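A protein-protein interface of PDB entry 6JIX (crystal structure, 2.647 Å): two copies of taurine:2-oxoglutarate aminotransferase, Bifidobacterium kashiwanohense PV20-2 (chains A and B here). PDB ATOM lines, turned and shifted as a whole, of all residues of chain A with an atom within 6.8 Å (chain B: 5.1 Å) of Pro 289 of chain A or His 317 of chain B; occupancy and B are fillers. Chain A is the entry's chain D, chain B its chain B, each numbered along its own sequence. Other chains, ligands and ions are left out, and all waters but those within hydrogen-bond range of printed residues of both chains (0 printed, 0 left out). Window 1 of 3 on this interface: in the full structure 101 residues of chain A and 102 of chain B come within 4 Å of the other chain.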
ATOM      1  N   THR A 113      11.055 -24.320  -0.728  1.00  0.00           N
ATOM      2  CA  THR A 113      10.083 -24.458   0.342  1.00  0.00           C
ATOM      3  C   THR A 113       8.730 -24.820  -0.264  1.00  0.00           C
ATOM      4  O   THR A 113       8.633 -25.060  -1.476  1.00  0.00           O
ATOM      5  CB  THR A 113      10.013 -23.158   1.166  1.00  0.00           C
ATOM      6  OG1 THR A 113       9.717 -22.056   0.305  1.00  0.00           O
ATOM      7  CG2 THR A 113      11.348 -22.865   1.877  1.00  0.00           C
ATOM      8  N   ASN A 114       7.681 -24.851   0.563  1.00  0.00           N
ATOM      9  CA  ASN A 114       6.341 -25.234   0.128  1.00  0.00           C
ATOM     10  C   ASN A 114       5.486 -24.064  -0.339  1.00  0.00           C
ATOM     11  O   ASN A 114       4.538 -24.280  -1.098  1.00  0.00           O
ATOM     12  CB  ASN A 114       5.585 -25.924   1.271  1.00  0.00           C
ATOM     13  CG  ASN A 114       6.002 -27.366   1.475  1.00  0.00           C
ATOM     14  OD1 ASN A 114       6.411 -28.047   0.537  1.00  0.00           O
ATOM     15  ND2 ASN A 114       5.895 -27.843   2.710  1.00  0.00           N
ATOM     16  N   GLY A 115       5.773 -22.849   0.097  1.00  0.00           N
ATOM     17  CA  GLY A 115       4.929 -21.737  -0.258  1.00  0.00           C
ATOM     18  C   GLY A 115       5.591 -20.443   0.121  1.00  0.00           C
ATOM     19  O   GLY A 115       6.812 -20.384   0.266  1.00  0.00           O
ATOM     20  N   VAL A 283       5.897 -19.432  -9.547  1.00  0.00           N
ATOM     21  CA  VAL A 283       6.935 -20.401  -9.879  1.00  0.00           C
ATOM     22  C   VAL A 283       6.329 -21.673 -10.454  1.00  0.00           C
ATOM     23  O   VAL A 283       6.974 -22.367 -11.243  1.00  0.00           O
ATOM     24  CB  VAL A 283       7.817 -20.704  -8.645  1.00  0.00           C
ATOM     25  CG1 VAL A 283       7.126 -21.681  -7.689  1.00  0.00           C
ATOM     26  CG2 VAL A 283       9.176 -21.241  -9.087  1.00  0.00           C
ATOM     27  N   THR A 284       5.111 -22.031 -10.045  1.00  0.00           N
ATOM     28  CA  THR A 284       4.414 -23.174 -10.634  1.00  0.00           C
ATOM     29  C   THR A 284       2.968 -22.841 -10.977  1.00  0.00           C
ATOM     30  O   THR A 284       2.182 -23.760 -11.244  1.00  0.00           O
ATOM     31  CB  THR A 284       4.423 -24.413  -9.725  1.00  0.00           C
ATOM     32  OG1 THR A 284       3.593 -24.155  -8.593  1.00  0.00           O
ATOM     33  CG2 THR A 284       5.807 -24.776  -9.258  1.00  0.00           C
ATOM     34  N   GLY A 286       0.706 -22.287  -9.135  1.00  0.00           N
ATOM     35  CA  GLY A 286      -0.138 -22.921  -8.147  1.00  0.00           C
ATOM     36  C   GLY A 286      -0.435 -24.380  -8.397  1.00  0.00           C
ATOM     37  O   GLY A 286      -1.156 -24.987  -7.596  1.00  0.00           O
ATOM     38  N   TYR A 287       0.093 -24.955  -9.485  1.00  0.00           N
ATOM     39  CA  TYR A 287      -0.210 -26.332  -9.868  1.00  0.00           C
ATOM     40  C   TYR A 287       0.362 -27.347  -8.887  1.00  0.00           C
ATOM     41  O   TYR A 287      -0.218 -28.424  -8.698  1.00  0.00           O
ATOM     42  CB  TYR A 287       0.341 -26.614 -11.262  1.00  0.00           C
ATOM     43  CG  TYR A 287      -0.360 -25.877 -12.374  1.00  0.00           C
ATOM     44  CD1 TYR A 287      -0.825 -24.571 -12.195  1.00  0.00           C
ATOM     45  CD2 TYR A 287      -0.564 -26.487 -13.608  1.00  0.00           C
ATOM     46  CE1 TYR A 287      -1.471 -23.894 -13.218  1.00  0.00           C
ATOM     47  CE2 TYR A 287      -1.206 -25.822 -14.636  1.00  0.00           C
ATOM     48  CZ  TYR A 287      -1.658 -24.526 -14.443  1.00  0.00           C
ATOM     49  OH  TYR A 287      -2.287 -23.867 -15.481  1.00  0.00           O
ATOM     50  N   VAL A 288       1.506 -27.042  -8.285  1.00  0.00           N
ATOM     51  CA  VAL A 288       2.056 -27.835  -7.192  1.00  0.00           C
ATOM     52  C   VAL A 288       2.652 -26.852  -6.194  1.00  0.00           C
ATOM     53  O   VAL A 288       3.288 -25.873  -6.605  1.00  0.00           O
ATOM     54  CB  VAL A 288       3.099 -28.851  -7.677  1.00  0.00           C
ATOM     55  CG1 VAL A 288       3.449 -29.801  -6.546  1.00  0.00           C
ATOM     56  CG2 VAL A 288       2.581 -29.606  -8.903  1.00  0.00           C
ATOM     57  N   PRO A 289       2.438 -27.043  -4.893  1.00  0.00           N
ATOM     58  CA  PRO A 289       2.992 -26.109  -3.902  1.00  0.00           C
ATOM     59  C   PRO A 289       4.511 -26.017  -3.993  1.00  0.00           C
ATOM     60  O   PRO A 289       5.211 -27.029  -3.941  1.00  0.00           O
ATOM     61  CB  PRO A 289       2.538 -26.719  -2.571  1.00  0.00           C
ATOM     62  CG  PRO A 289       1.273 -27.447  -2.927  1.00  0.00           C
ATOM     63  CD  PRO A 289       1.532 -28.028  -4.278  1.00  0.00           C
ATOM     64  N   LEU A 290       5.020 -24.794  -4.143  1.00  0.00           N
ATOM     65  CA  LEU A 290       6.461 -24.569  -4.169  1.00  0.00           C
ATOM     66  C   LEU A 290       6.759 -23.094  -3.903  1.00  0.00           C
ATOM     67  O   LEU A 290       6.074 -22.204  -4.415  1.00  0.00           O
ATOM     68  CB  LEU A 290       7.068 -25.007  -5.510  1.00  0.00           C
ATOM     69  CG  LEU A 290       8.585 -24.907  -5.698  1.00  0.00           C
ATOM     70  CD1 LEU A 290       9.349 -25.894  -4.819  1.00  0.00           C
ATOM     71  CD2 LEU A 290       8.946 -25.137  -7.151  1.00  0.00           C
ATOM     72  N   GLY A 291       7.778 -22.849  -3.101  1.00  0.00           N
ATOM     73  CA  GLY A 291       8.257 -21.507  -2.848  1.00  0.00           C
ATOM     74  C   GLY A 291       9.757 -21.594  -2.708  1.00  0.00           C
ATOM     75  O   GLY A 291      10.325 -22.656  -2.973  1.00  0.00           O
ATOM     76  N   TYR A 314       9.714 -31.534   2.651  1.00  0.00           N
ATOM     77  CA  TYR A 314       9.406 -31.443   1.228  1.00  0.00           C
ATOM     78  C   TYR A 314      10.273 -30.432   0.474  1.00  0.00           C
ATOM     79  O   TYR A 314       9.920 -30.064  -0.651  1.00  0.00           O
ATOM     80  CB  TYR A 314       7.919 -31.111   1.053  1.00  0.00           C
ATOM     81  CG  TYR A 314       7.004 -32.237   1.490  1.00  0.00           C
ATOM     82  CD1 TYR A 314       7.382 -33.582   1.330  1.00  0.00           C
ATOM     83  CD2 TYR A 314       5.766 -31.968   2.067  1.00  0.00           C
ATOM     84  CE1 TYR A 314       6.539 -34.630   1.736  1.00  0.00           C
ATOM     85  CE2 TYR A 314       4.923 -32.999   2.478  1.00  0.00           C
ATOM     86  CZ  TYR A 314       5.310 -34.332   2.302  1.00  0.00           C
ATOM     87  OH  TYR A 314       4.459 -35.348   2.689  1.00  0.00           O
ATOM     88  N   HIS A 317      10.739 -30.358  -3.414  1.00  0.00           N
ATOM     89  CA  HIS A 317       9.870 -31.452  -3.818  1.00  0.00           C
ATOM     90  C   HIS A 317       9.966 -31.690  -5.322  1.00  0.00           C
ATOM     91  O   HIS A 317       9.832 -30.761  -6.130  1.00  0.00           O
ATOM     92  CB  HIS A 317       8.431 -31.131  -3.406  1.00  0.00           C
ATOM     93  CG  HIS A 317       7.464 -32.235  -3.672  1.00  0.00           C
ATOM     94  ND1 HIS A 317       6.921 -32.458  -4.920  1.00  0.00           N
ATOM     95  CD2 HIS A 317       6.956 -33.195  -2.859  1.00  0.00           C
ATOM     96  CE1 HIS A 317       6.109 -33.503  -4.860  1.00  0.00           C
ATOM     97  NE2 HIS A 317       6.115 -33.968  -3.623  1.00  0.00           N
ATOM     98  N   ALA A 320       7.009 -30.941  -7.670  1.00  0.00           N
ATOM     99  CA  ALA A 320       6.831 -29.492  -7.672  1.00  0.00           C
ATOM    100  C   ALA A 320       7.879 -28.803  -8.543  1.00  0.00           C
ATOM    101  O   ALA A 320       7.551 -27.931  -9.365  1.00  0.00           O
ATOM    102  CB  ALA A 320       6.881 -28.959  -6.239  1.00  0.00           C
ATOM    103  N   CYS A 321       9.148 -29.201  -8.403  1.00  0.00           N
ATOM    104  CA  CYS A 321      10.192 -28.577  -9.209  1.00  0.00           C
ATOM    105  C   CYS A 321       9.994 -28.862 -10.694  1.00  0.00           C
ATOM    106  O   CYS A 321      10.188 -27.971 -11.535  1.00  0.00           O
ATOM    107  CB  CYS A 321      11.567 -29.044  -8.749  1.00  0.00           C
ATOM    108  SG  CYS A 321      12.108 -28.358  -7.161  1.00  0.00           S
ATOM    109  N   CYS B  80      -5.456 -28.649 -11.687  1.00  0.00           N
ATOM    110  CA  CYS B  80      -4.341 -28.825 -10.755  1.00  0.00           C
ATOM    111  C   CYS B  80      -4.568 -28.065  -9.448  1.00  0.00           C
ATOM    112  O   CYS B  80      -4.174 -28.541  -8.375  1.00  0.00           O
ATOM    113  CB  CYS B  80      -3.030 -28.369 -11.396  1.00  0.00           C
ATOM    114  SG  CYS B  80      -2.367 -29.480 -12.662  1.00  0.00           S
ATOM    115  N   PHE B  81      -5.154 -26.863  -9.526  1.00  0.00           N
ATOM    116  CA  PHE B  81      -5.395 -26.019  -8.364  1.00  0.00           C
ATOM    117  C   PHE B  81      -6.655 -25.189  -8.563  1.00  0.00           C
ATOM    118  O   PHE B  81      -6.914 -24.692  -9.661  1.00  0.00           O
ATOM    119  CB  PHE B  81      -4.225 -25.072  -8.076  1.00  0.00           C
ATOM    120  CG  PHE B  81      -4.422 -24.235  -6.838  1.00  0.00           C
ATOM    121  CD1 PHE B  81      -4.569 -24.835  -5.592  1.00  0.00           C
ATOM    122  CD2 PHE B  81      -4.477 -22.848  -6.921  1.00  0.00           C
ATOM    123  CE1 PHE B  81      -4.751 -24.070  -4.449  1.00  0.00           C
ATOM    124  CE2 PHE B  81      -4.667 -22.073  -5.788  1.00  0.00           C
ATOM    125  CZ  PHE B  81      -4.804 -22.686  -4.545  1.00  0.00           C
ATOM    126  N   ASN B 114       0.265 -27.210   3.862  1.00  0.00           N
ATOM    127  CA  ASN B 114       1.233 -27.722   2.909  1.00  0.00           C
ATOM    128  C   ASN B 114       2.126 -28.813   3.469  1.00  0.00           C
ATOM    129  O   ASN B 114       2.770 -29.519   2.685  1.00  0.00           O
ATOM    130  CB  ASN B 114       2.091 -26.582   2.374  1.00  0.00           C
ATOM    131  CG  ASN B 114       1.347 -25.758   1.368  1.00  0.00           C
ATOM    132  OD1 ASN B 114       0.496 -26.291   0.657  1.00  0.00           O
ATOM    133  ND2 ASN B 114       1.625 -24.452   1.318  1.00  0.00           N
ATOM    134  N   VAL B 288       2.676 -35.427  -3.146  1.00  0.00           N
ATOM    135  CA  VAL B 288       2.343 -34.008  -3.297  1.00  0.00           C
ATOM    136  C   VAL B 288       2.317 -33.394  -1.904  1.00  0.00           C
ATOM    137  O   VAL B 288       1.748 -34.005  -0.985  1.00  0.00           O
ATOM    138  CB  VAL B 288       0.988 -33.805  -3.993  1.00  0.00           C
ATOM    139  CG1 VAL B 288       0.757 -32.320  -4.313  1.00  0.00           C
ATOM    140  CG2 VAL B 288       0.899 -34.656  -5.235  1.00  0.00           C
ATOM    141  N   PRO B 289       2.898 -32.207  -1.701  1.00  0.00           N
ATOM    142  CA  PRO B 289       2.900 -31.589  -0.362  1.00  0.00           C
ATOM    143  C   PRO B 289       1.487 -31.411   0.176  1.00  0.00           C
ATOM    144  O   PRO B 289       0.644 -30.751  -0.441  1.00  0.00           O
ATOM    145  CB  PRO B 289       3.580 -30.238  -0.605  1.00  0.00           C
ATOM    146  CG  PRO B 289       4.474 -30.491  -1.759  1.00  0.00           C
ATOM    147  CD  PRO B 289       3.742 -31.463  -2.649  1.00  0.00           C
ATOM    148  N   TYR B 314      -2.280 -22.059  -0.628  1.00  0.00           N
ATOM    149  CA  TYR B 314      -2.490 -23.381  -1.213  1.00  0.00           C
ATOM    150  C   TYR B 314      -3.340 -24.323  -0.344  1.00  0.00           C
ATOM    151  O   TYR B 314      -3.404 -25.516  -0.647  1.00  0.00           O
ATOM    152  CB  TYR B 314      -1.139 -24.045  -1.527  1.00  0.00           C
ATOM    153  CG  TYR B 314      -0.325 -23.370  -2.628  1.00  0.00           C
ATOM    154  CD1 TYR B 314      -0.943 -22.643  -3.657  1.00  0.00           C
ATOM    155  CD2 TYR B 314       1.068 -23.455  -2.634  1.00  0.00           C
ATOM    156  CE1 TYR B 314      -0.187 -22.017  -4.660  1.00  0.00           C
ATOM    157  CE2 TYR B 314       1.828 -22.832  -3.623  1.00  0.00           C
ATOM    158  CZ  TYR B 314       1.200 -22.117  -4.637  1.00  0.00           C
ATOM    159  OH  TYR B 314       1.976 -21.526  -5.624  1.00  0.00           O
ATOM    160  N   SER B 315      -3.997 -23.828   0.715  1.00  0.00           N
ATOM    161  CA  SER B 315      -4.785 -24.695   1.605  1.00  0.00           C
ATOM    162  C   SER B 315      -5.823 -25.507   0.836  1.00  0.00           C
ATOM    163  O   SER B 315      -6.582 -24.956   0.037  1.00  0.00           O
ATOM    164  CB  SER B 315      -5.483 -23.864   2.683  1.00  0.00           C
ATOM    165  OG  SER B 315      -6.319 -24.686   3.483  1.00  0.00           O
ATOM    166  N   GLY B 316      -5.875 -26.811   1.098  1.00  0.00           N
ATOM    167  CA  GLY B 316      -6.801 -27.666   0.375  1.00  0.00           C
ATOM    168  C   GLY B 316      -6.444 -27.824  -1.083  1.00  0.00           C
ATOM    169  O   GLY B 316      -7.330 -27.997  -1.929  1.00  0.00           O
ATOM    170  N   HIS B 317      -5.153 -27.765  -1.392  1.00  0.00           N
ATOM    171  CA  HIS B 317      -4.664 -27.844  -2.753  1.00  0.00           C
ATOM    172  C   HIS B 317      -5.286 -29.023  -3.488  1.00  0.00           C
ATOM    173  O   HIS B 317      -5.305 -30.149  -2.988  1.00  0.00           O
ATOM    174  CB  HIS B 317      -3.144 -27.961  -2.704  1.00  0.00           C
ATOM    175  CG  HIS B 317      -2.482 -27.815  -4.037  1.00  0.00           C
ATOM    176  ND1 HIS B 317      -2.496 -28.817  -4.987  1.00  0.00           N
ATOM    177  CD2 HIS B 317      -1.787 -26.786  -4.578  1.00  0.00           C
ATOM    178  CE1 HIS B 317      -1.837 -28.405  -6.058  1.00  0.00           C
ATOM    179  NE2 HIS B 317      -1.392 -27.179  -5.834  1.00  0.00           N
ATOM    180  N   THR B 318      -5.793 -28.760  -4.687  1.00  0.00           N
ATOM    181  CA  THR B 318      -6.634 -29.745  -5.362  1.00  0.00           C
ATOM    182  C   THR B 318      -5.842 -30.978  -5.776  1.00  0.00           C
ATOM    183  O   THR B 318      -6.222 -32.105  -5.438  1.00  0.00           O
ATOM    184  CB  THR B 318      -7.325 -29.097  -6.556  1.00  0.00           C
ATOM    185  OG1 THR B 318      -7.812 -27.812  -6.145  1.00  0.00           O
ATOM    186  CG2 THR B 318      -8.514 -29.941  -7.013  1.00  0.00           C
ATOM    187  N   LEU B 319      -4.744 -30.799  -6.511  1.00  0.00           N
ATOM    188  CA  LEU B 319      -3.901 -31.947  -6.851  1.00  0.00           C
ATOM    189  C   LEU B 319      -3.490 -32.713  -5.602  1.00  0.00           C
ATOM    190  O   LEU B 319      -3.603 -33.938  -5.539  1.00  0.00           O
ATOM    191  CB  LEU B 319      -2.660 -31.493  -7.613  1.00  0.00           C
ATOM    192  CG  LEU B 319      -1.976 -32.619  -8.373  1.00  0.00           C
ATOM    193  CD1 LEU B 319      -2.702 -32.863  -9.682  1.00  0.00           C
ATOM    194  CD2 LEU B 319      -0.504 -32.297  -8.597  1.00  0.00           C
ATOM    195  N   ALA B 320      -3.015 -31.995  -4.587  1.00  0.00           N
ATOM    196  CA  ALA B 320      -2.532 -32.653  -3.386  1.00  0.00           C
ATOM    197  C   ALA B 320      -3.628 -33.496  -2.763  1.00  0.00           C
ATOM    198  O   ALA B 320      -3.384 -34.633  -2.348  1.00  0.00           O
ATOM    199  CB  ALA B 320      -2.016 -31.615  -2.389  1.00  0.00           C
ATOM    200  N   CYS B 321      -4.849 -32.950  -2.694  1.00  0.00           N
ATOM    201  CA  CYS B 321      -5.969 -33.687  -2.115  1.00  0.00           C
ATOM    202  C   CYS B 321      -6.314 -34.917  -2.935  1.00  0.00           C
ATOM    203  O   CYS B 321      -6.593 -35.982  -2.366  1.00  0.00           O
ATOM    204  CB  CYS B 321      -7.184 -32.781  -1.987  1.00  0.00           C
ATOM    205  SG  CYS B 321      -7.064 -31.668  -0.600  1.00  0.00           S
ATOM    206  N   ALA B 322      -6.318 -34.792  -4.271  1.00  0.00           N
ATOM    207  CA  ALA B 322      -6.567 -35.958  -5.117  1.00  0.00           C
ATOM    208  C   ALA B 322      -5.581 -37.074  -4.792  1.00  0.00           C
ATOM    209  O   ALA B 322      -5.970 -38.240  -4.639  1.00  0.00           O
ATOM    210  CB  ALA B 322      -6.498 -35.584  -6.600  1.00  0.00           C
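Printed residues of chain B within 4 Å of Pro 289 of chain A: Asn 114, Tyr 314 and His 317. Of the printed residues of chain A, His 317 of chain B touches Gly 286 (2.8 Å), Tyr 287 (3.1 Å), Val 288 (3.8 Å) and Pro 289 (3.4 Å). Of the printed residues of chain B, Tyr 314 of chain A touches Asn 114 (3.9 Å) and Pro 289 (3.8 Å). Printed residues of chain B within 4 Å of Gly 286 of chain A: Phe 81 (3.1 Å), Tyr 314 (3.6 Å) and His 317 (2.8 Å). Thr 284 of chain A touches none of the printed residues of chain B. Gly 316 of chain B touches none of the printed residues of chain A. The nearest residue of chain A that does not touch His 317 of chain B is Thr 284 of chain A (6.5 Å). The nearest printed residue of chain A that does not touch Leu 319 of chain B is Val 288 of chain A (4.1 Å).
Along chain A the printed residues that touch a printed residue of chain B span positions 114 to 317. Among the printed residues, 18 pairs touch across the chains. Among the printed residues, no Asp or Glu carboxylate lies within 4 Å of a Lys or Arg side-chain nitrogen of the other chain.
NE2 of His 317 of chain B sits close to O of Tyr 287 of chain A (3.3 Å). A ring nitrogen (NE2) of His 317 of chain B is in hydrogen-bond range of the backbone carbonyl oxygen (O) of Gly 286 of chain A, at 2.8 Å.
Asn 114 of chain B touches Asn 114 of chain A (O to ND2, 3.5 Å). Asn 114 of chain A touches Tyr 314 of chain B (O to CD2, 3.9 Å). Gly 286 of chain A touches Tyr 314 of chain B. CA of Val 288 of chain A touches NE2 of His 317 of chain B (3.8 Å). Tyr 314 of chain B touches Pro 289 of chain A. His 317 of chain B touches Pro 289 of chain A (NE2 to CD, 3.4 Å). Asn 114 of chain B touches Tyr 314 of chain A (O to CD2, 3.9 Å). Tyr 314 of chain A touches Pro 289 of chain B (CE2 to CA, 3.8 Å). His 317 of chain A touches Val 288 of chain B (NE2 to N, 3.8 Å). CD of Pro 289 of chain B touches NE2 of His 317 of chain A (3.6 Å).
Asn 114 of chain A touches its own counterpart, Asn 114 of chain B. Asn 114 of chain A touches Tyr 314 of chain B, and with the chains exchanged Tyr 314 of chain A touches Asn 114 of chain B. Val 288 of chain A touches His 317 of chain B, and with the chains exchanged His 317 of chain A touches Val 288 of chain B. Pro 289 of chain A touches Tyr 314 of chain B, and with the chains exchanged Tyr 314 of chain A touches Pro 289 of chain B. Positions printed for both chains: 114, 288, 289, 314, 317, 320 and 321. Of the 18 pairs that touch across the chains among the printed residues, 11 have their exchanged pair printed and touching as well.
The backbone NH of Leu 319 of chain B is in hydrogen-bond range of the backbone carbonyl oxygen of Cys 80 of chain B (3.0 Å). ND1 of His 317 of chain A is in hydrogen-bond range of N of Ala 320 of chain A (3.1 Å). N of Leu 319 of chain B sits at hydrogen-bond distance from ND1 of His 317 of chain B (3.4 Å). The side-chain hydroxyl of Thr 284 of chain A sits at hydrogen-bond distance from the backbone carbonyl oxygen of Val 288 of chain A (2.6 Å). The side-chain hydroxyl (OG1) of Thr 284 of chain A lies close to the backbone NH (N) of Gly 286 of chain A, 3.5 Å away. The backbone carbonyl oxygen (O) of His 317 of chain B sits at hydrogen-bond distance from the side-chain sulfur (SG) of Cys 321 of chain B (3.3 Å).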
